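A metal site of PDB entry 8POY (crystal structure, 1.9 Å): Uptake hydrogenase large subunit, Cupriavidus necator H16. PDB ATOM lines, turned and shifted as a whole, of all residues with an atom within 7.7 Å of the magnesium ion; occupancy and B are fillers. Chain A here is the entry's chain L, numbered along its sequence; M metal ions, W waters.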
ATOM      1  N   TRP A  52      21.291  33.907   5.091  1.00  0.00           N
ATOM      2  CA  TRP A  52      22.706  33.789   4.767  1.00  0.00           C
ATOM      3  C   TRP A  52      23.494  34.729   5.666  1.00  0.00           C
ATOM      4  O   TRP A  52      23.019  35.817   5.987  1.00  0.00           O
ATOM      5  CB  TRP A  52      22.962  34.114   3.292  1.00  0.00           C
ATOM      6  CG  TRP A  52      24.395  34.000   2.881  1.00  0.00           C
ATOM      7  CD1 TRP A  52      25.175  32.882   2.910  1.00  0.00           C
ATOM      8  CD2 TRP A  52      25.236  35.062   2.379  1.00  0.00           C
ATOM      9  NE1 TRP A  52      26.430  33.165   2.460  1.00  0.00           N
ATOM     10  CE2 TRP A  52      26.508  34.494   2.129  1.00  0.00           C
ATOM     11  CE3 TRP A  52      25.040  36.417   2.129  1.00  0.00           C
ATOM     12  CZ2 TRP A  52      27.569  35.234   1.640  1.00  0.00           C
ATOM     13  CZ3 TRP A  52      26.106  37.165   1.639  1.00  0.00           C
ATOM     14  CH2 TRP A  52      27.357  36.565   1.396  1.00  0.00           C
ATOM     15  N   GLU A  56      32.073  32.050   4.945  1.00  0.00           N
ATOM     16  CA  GLU A  56      33.181  31.739   4.043  1.00  0.00           C
ATOM     17  C   GLU A  56      33.923  33.003   3.613  1.00  0.00           C
ATOM     18  O   GLU A  56      35.139  32.994   3.462  1.00  0.00           O
ATOM     19  CB  GLU A  56      32.658  30.965   2.825  1.00  0.00           C
ATOM     20  CG  GLU A  56      32.109  29.585   3.187  1.00  0.00           C
ATOM     21  CD  GLU A  56      31.132  29.030   2.165  1.00  0.00           C
ATOM     22  OE1 GLU A  56      30.457  29.834   1.503  1.00  0.00           O
ATOM     23  OE2 GLU A  56      31.025  27.784   2.045  1.00  0.00           O
ATOM     24  N   GLU A 347      29.600  22.224  -6.504  1.00  0.00           N
ATOM     25  CA  GLU A 347      28.431  23.011  -6.175  1.00  0.00           C
ATOM     26  C   GLU A 347      28.037  23.919  -7.324  1.00  0.00           C
ATOM     27  O   GLU A 347      28.866  24.682  -7.838  1.00  0.00           O
ATOM     28  CB  GLU A 347      28.695  23.847  -4.942  1.00  0.00           C
ATOM     29  CG  GLU A 347      28.822  23.030  -3.677  1.00  0.00           C
ATOM     30  CD  GLU A 347      28.974  23.919  -2.474  1.00  0.00           C
ATOM     31  OE1 GLU A 347      29.991  24.637  -2.404  1.00  0.00           O
ATOM     32  OE2 GLU A 347      28.059  23.900  -1.616  1.00  0.00           O
ATOM     33  N   TYR A 354      23.638  33.394  -5.750  1.00  0.00           N
ATOM     34  CA  TYR A 354      25.079  33.593  -5.839  1.00  0.00           C
ATOM     35  C   TYR A 354      25.444  33.729  -7.301  1.00  0.00           C
ATOM     36  O   TYR A 354      24.626  33.422  -8.177  1.00  0.00           O
ATOM     37  CB  TYR A 354      25.857  32.433  -5.223  1.00  0.00           C
ATOM     38  CG  TYR A 354      25.507  32.135  -3.786  1.00  0.00           C
ATOM     39  CD1 TYR A 354      26.063  32.858  -2.744  1.00  0.00           C
ATOM     40  CD2 TYR A 354      24.601  31.131  -3.476  1.00  0.00           C
ATOM     41  CE1 TYR A 354      25.730  32.595  -1.424  1.00  0.00           C
ATOM     42  CE2 TYR A 354      24.263  30.857  -2.168  1.00  0.00           C
ATOM     43  CZ  TYR A 354      24.825  31.584  -1.141  1.00  0.00           C
ATOM     44  OH  TYR A 354      24.487  31.306   0.153  1.00  0.00           O
ATOM     45  N   PRO A 365      34.991  22.510  -4.027  1.00  0.00           N
ATOM     46  CA  PRO A 365      35.107  23.554  -2.988  1.00  0.00           C
ATOM     47  C   PRO A 365      36.485  24.203  -2.783  1.00  0.00           C
ATOM     48  O   PRO A 365      36.548  25.347  -2.339  1.00  0.00           O
ATOM     49  CB  PRO A 365      34.662  22.828  -1.723  1.00  0.00           C
ATOM     50  CG  PRO A 365      33.799  21.707  -2.206  1.00  0.00           C
ATOM     51  CD  PRO A 365      34.450  21.253  -3.477  1.00  0.00           C
ATOM     52  N   VAL A 369      33.502  29.608  -4.800  1.00  0.00           N
ATOM     53  CA  VAL A 369      33.328  31.053  -4.816  1.00  0.00           C
ATOM     54  C   VAL A 369      32.009  31.349  -4.142  1.00  0.00           C
ATOM     55  O   VAL A 369      31.003  30.684  -4.422  1.00  0.00           O
ATOM     56  CB  VAL A 369      33.322  31.590  -6.263  1.00  0.00           C
ATOM     57  CG1 VAL A 369      32.910  33.060  -6.314  1.00  0.00           C
ATOM     58  CG2 VAL A 369      34.693  31.390  -6.902  1.00  0.00           C
ATOM     59  N   THR A 370      32.002  32.330  -3.243  1.00  0.00           N
ATOM     60  CA  THR A 370      30.776  32.730  -2.548  1.00  0.00           C
ATOM     61  C   THR A 370      30.583  34.224  -2.716  1.00  0.00           C
ATOM     62  O   THR A 370      31.091  35.026  -1.935  1.00  0.00           O
ATOM     63  CB  THR A 370      30.796  32.338  -1.064  1.00  0.00           C
ATOM     64  OG1 THR A 370      31.037  30.931  -0.961  1.00  0.00           O
ATOM     65  CG2 THR A 370      29.468  32.690  -0.382  1.00  0.00           C
ATOM     66  N   TRP A 398      19.153  30.693  -0.826  1.00  0.00           N
ATOM     67  CA  TRP A 398      20.490  30.990  -0.322  1.00  0.00           C
ATOM     68  C   TRP A 398      21.347  29.737  -0.192  1.00  0.00           C
ATOM     69  O   TRP A 398      22.512  29.824   0.186  1.00  0.00           O
ATOM     70  CB  TRP A 398      20.408  31.703   1.036  1.00  0.00           C
ATOM     71  CG  TRP A 398      20.032  33.158   0.917  1.00  0.00           C
ATOM     72  CD1 TRP A 398      18.879  33.736   1.335  1.00  0.00           C
ATOM     73  CD2 TRP A 398      20.822  34.196   0.333  1.00  0.00           C
ATOM     74  NE1 TRP A 398      18.897  35.091   1.054  1.00  0.00           N
ATOM     75  CE2 TRP A 398      20.066  35.390   0.431  1.00  0.00           C
ATOM     76  CE3 TRP A 398      22.076  34.224  -0.279  1.00  0.00           C
ATOM     77  CZ2 TRP A 398      20.545  36.607  -0.045  1.00  0.00           C
ATOM     78  CZ3 TRP A 398      22.555  35.441  -0.755  1.00  0.00           C
ATOM     79  CH2 TRP A 398      21.782  36.614  -0.637  1.00  0.00           C
ATOM     80  N   LYS A 400      23.411  26.656  -1.871  1.00  0.00           N
ATOM     81  CA  LYS A 400      24.033  26.196  -3.097  1.00  0.00           C
ATOM     82  C   LYS A 400      23.544  24.782  -3.432  1.00  0.00           C
ATOM     83  O   LYS A 400      22.849  24.158  -2.629  1.00  0.00           O
ATOM     84  CB  LYS A 400      25.559  26.204  -2.990  1.00  0.00           C
ATOM     85  CG  LYS A 400      26.161  27.591  -2.820  1.00  0.00           C
ATOM     86  CD  LYS A 400      27.675  27.504  -2.792  1.00  0.00           C
ATOM     87  CE  LYS A 400      28.337  28.867  -2.709  1.00  0.00           C
ATOM     88  NZ  LYS A 400      29.806  28.725  -2.522  1.00  0.00           N
ATOM     89  N   PRO A 402      24.931  21.261  -4.150  1.00  0.00           N
ATOM     90  CA  PRO A 402      25.990  20.258  -4.260  1.00  0.00           C
ATOM     91  C   PRO A 402      25.541  19.021  -5.025  1.00  0.00           C
ATOM     92  O   PRO A 402      24.397  18.571  -4.873  1.00  0.00           O
ATOM     93  CB  PRO A 402      26.302  19.900  -2.806  1.00  0.00           C
ATOM     94  CG  PRO A 402      25.557  20.863  -1.950  1.00  0.00           C
ATOM     95  CD  PRO A 402      24.399  21.333  -2.781  1.00  0.00           C
ATOM     96  N   GLY A 534      31.777  18.641   4.903  1.00  0.00           N
ATOM     97  CA  GLY A 534      33.167  18.877   4.519  1.00  0.00           C
ATOM     98  C   GLY A 534      33.557  20.337   4.622  1.00  0.00           C
ATOM     99  O   GLY A 534      32.747  21.212   4.303  1.00  0.00           O
ATOM    100  N   TYR A 547      38.153  29.452   2.074  1.00  0.00           N
ATOM    101  CA  TYR A 547      37.531  28.531   3.004  1.00  0.00           C
ATOM    102  C   TYR A 547      36.128  28.266   2.505  1.00  0.00           C
ATOM    103  O   TYR A 547      35.331  29.180   2.439  1.00  0.00           O
ATOM    104  CB  TYR A 547      37.514  29.106   4.420  1.00  0.00           C
ATOM    105  CG  TYR A 547      37.402  28.048   5.499  1.00  0.00           C
ATOM    106  CD1 TYR A 547      36.228  27.305   5.665  1.00  0.00           C
ATOM    107  CD2 TYR A 547      38.479  27.778   6.337  1.00  0.00           C
ATOM    108  CE1 TYR A 547      36.141  26.329   6.644  1.00  0.00           C
ATOM    109  CE2 TYR A 547      38.403  26.805   7.308  1.00  0.00           C
ATOM    110  CZ  TYR A 547      37.223  26.077   7.470  1.00  0.00           C
ATOM    111  OH  TYR A 547      37.153  25.112   8.439  1.00  0.00           O
ATOM    112  N   GLN A 548      35.850  27.012   2.142  1.00  0.00           N
ATOM    113  CA  GLN A 548      34.535  26.638   1.628  1.00  0.00           C
ATOM    114  C   GLN A 548      33.952  25.458   2.392  1.00  0.00           C
ATOM    115  O   GLN A 548      34.610  24.434   2.584  1.00  0.00           O
ATOM    116  CB  GLN A 548      34.632  26.296   0.134  1.00  0.00           C
ATOM    117  CG  GLN A 548      34.897  27.484  -0.748  1.00  0.00           C
ATOM    118  CD  GLN A 548      33.690  28.399  -0.904  1.00  0.00           C
ATOM    119  OE1 GLN A 548      32.573  27.930  -1.119  1.00  0.00           O
ATOM    120  NE2 GLN A 548      33.911  29.681  -0.834  1.00  0.00           N
ATOM    121  N   CYS A 549      32.685  25.608   2.791  1.00  0.00           N
ATOM    122  CA  CYS A 549      31.963  24.554   3.497  1.00  0.00           C
ATOM    123  C   CYS A 549      30.865  23.985   2.600  1.00  0.00           C
ATOM    124  O   CYS A 549      30.141  24.735   1.935  1.00  0.00           O
ATOM    125  CB  CYS A 549      31.335  25.116   4.778  1.00  0.00           C
ATOM    126  SG  CYS A 549      32.479  25.963   5.898  1.00  0.00           S
ATOM    127  N   VAL A 550      30.762  22.658   2.559  1.00  0.00           N
ATOM    128  CA  VAL A 550      29.609  21.975   2.003  1.00  0.00           C
ATOM    129  C   VAL A 550      29.004  21.121   3.114  1.00  0.00           C
ATOM    130  O   VAL A 550      29.642  20.197   3.623  1.00  0.00           O
ATOM    131  CB  VAL A 550      29.959  21.107   0.777  1.00  0.00           C
ATOM    132  CG1 VAL A 550      28.701  20.558   0.141  1.00  0.00           C
ATOM    133  CG2 VAL A 550      30.755  21.921  -0.232  1.00  0.00           C
ATOM    134  N   VAL A 551      27.770  21.420   3.461  1.00  0.00           N
ATOM    135  CA  VAL A 551      27.184  21.030   4.734  1.00  0.00           C
ATOM    136  C   VAL A 551      25.990  20.107   4.441  1.00  0.00           C
ATOM    137  O   VAL A 551      25.431  20.164   3.349  1.00  0.00           O
ATOM    138  CB  VAL A 551      26.809  22.315   5.496  1.00  0.00           C
ATOM    139  CG1 VAL A 551      26.285  22.035   6.889  1.00  0.00           C
ATOM    140  CG2 VAL A 551      28.023  23.228   5.595  1.00  0.00           C
ATOM    141  N   THR A 554      22.931  21.557   3.108  1.00  0.00           N
ATOM    142  CA  THR A 554      23.225  22.096   1.769  1.00  0.00           C
ATOM    143  C   THR A 554      22.908  21.031   0.709  1.00  0.00           C
ATOM    144  O   THR A 554      22.265  21.322  -0.291  1.00  0.00           O
ATOM    145  CB  THR A 554      24.687  22.554   1.601  1.00  0.00           C
ATOM    146  OG1 THR A 554      25.101  23.317   2.733  1.00  0.00           O
ATOM    147  CG2 THR A 554      24.860  23.382   0.333  1.00  0.00           C
ATOM    148  N   CYS A 600      23.197  25.958   9.018  1.00  0.00           N
ATOM    149  CA  CYS A 600      24.179  25.046   8.468  1.00  0.00           C
ATOM    150  C   CYS A 600      24.193  25.058   6.956  1.00  0.00           C
ATOM    151  O   CYS A 600      25.265  25.118   6.346  1.00  0.00           O
ATOM    152  CB  CYS A 600      23.903  23.612   8.945  1.00  0.00           C
ATOM    153  SG  CYS A 600      24.942  23.115  10.312  1.00  0.00           S
ATOM    154  N   SER A 601      23.012  24.976   6.350  1.00  0.00           N
ATOM    155  CA  SER A 601      22.908  24.813   4.908  1.00  0.00           C
ATOM    156  C   SER A 601      23.495  26.005   4.157  1.00  0.00           C
ATOM    157  O   SER A 601      24.047  25.840   3.067  1.00  0.00           O
ATOM    158  CB  SER A 601      21.456  24.584   4.479  1.00  0.00           C
ATOM    159  OG  SER A 601      20.688  25.775   4.585  1.00  0.00           O
ATOM    160  N   THR A 602      23.393  27.183   4.756  1.00  0.00           N
ATOM    161  CA  THR A 602      23.774  28.433   4.094  1.00  0.00           C
ATOM    162  C   THR A 602      25.094  29.031   4.595  1.00  0.00           C
ATOM    163  O   THR A 602      25.851  29.581   3.805  1.00  0.00           O
ATOM    164  CB  THR A 602      22.644  29.469   4.252  1.00  0.00           C
ATOM    165  OG1 THR A 602      22.348  29.650   5.651  1.00  0.00           O
ATOM    166  CG2 THR A 602      21.400  28.989   3.534  1.00  0.00           C
ATOM    167  N   HIS A 603      25.336  28.929   5.910  1.00  0.00           N
ATOM    168  CA  HIS A 603      26.563  29.425   6.544  1.00  0.00           C
ATOM    169  C   HIS A 603      27.009  30.813   6.032  1.00  0.00           C
ATOM    170  O   HIS A 603      28.171  31.091   5.713  1.00  0.00           O
ATOM    171  CB  HIS A 603      27.698  28.384   6.482  1.00  0.00           C
ATOM    172  CG  HIS A 603      27.803  27.670   5.184  1.00  0.00           C
ATOM    173  ND1 HIS A 603      26.994  26.598   4.850  1.00  0.00           N
ATOM    174  CD2 HIS A 603      28.582  27.894   4.096  1.00  0.00           C
ATOM    175  CE1 HIS A 603      27.295  26.189   3.632  1.00  0.00           C
ATOM    176  NE2 HIS A 603      28.251  26.950   3.151  1.00  0.00           N
ATOM    177  OXT HIS A 603      26.167  31.715   5.946  1.00  0.00           O
HETATM  178 MG    MG M   1      29.366  26.593   1.094  1.00  0.00          MG
HETATM  179  O   HOH W   1      27.677  25.487   0.463  1.00  0.00           O
HETATM  180  O   HOH W   2      30.598  26.232  -0.405  1.00  0.00           O
HETATM  181  O   HOH W   3      28.485  28.370   0.438  1.00  0.00           O
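OG1 of Thr 370 lies within hydrogen-bond range of OE1 of Glu 56 (2.8 Å).
A ring nitrogen (ND1) of His 603 is in hydrogen-bond range of the backbone carbonyl oxygen (O) of Cys 600.
Within 4 Å of the magnesium ion: Glu 56, Cys 549 and His 603.
The magnesium ion is bound by water W2 (2.0 Å), water W3 (2.1 Å), water W1 (2.1 Å), the backbone carbonyl oxygen of Cys 549 (2.2 Å), the side-chain carboxylate of Glu 56 (2.3 Å) and a ring nitrogen (NE2) of His 603 (2.4 Å).
The magnesium ion has six donor atoms within binding distance.
Water W3 bridges OE1 of Glu 56 (2.7 Å) and NZ of Lys 400 (3.3 Å).
Water W2 lies within hydrogen-bond range of the side-chain carboxylate (OE1) of Glu 347 (2.6 Å), the side-chain amide oxygen (OE1) of Gln 548 (2.7 Å) and the side-chain amino group (NZ) of Lys 400 (3.4 Å).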
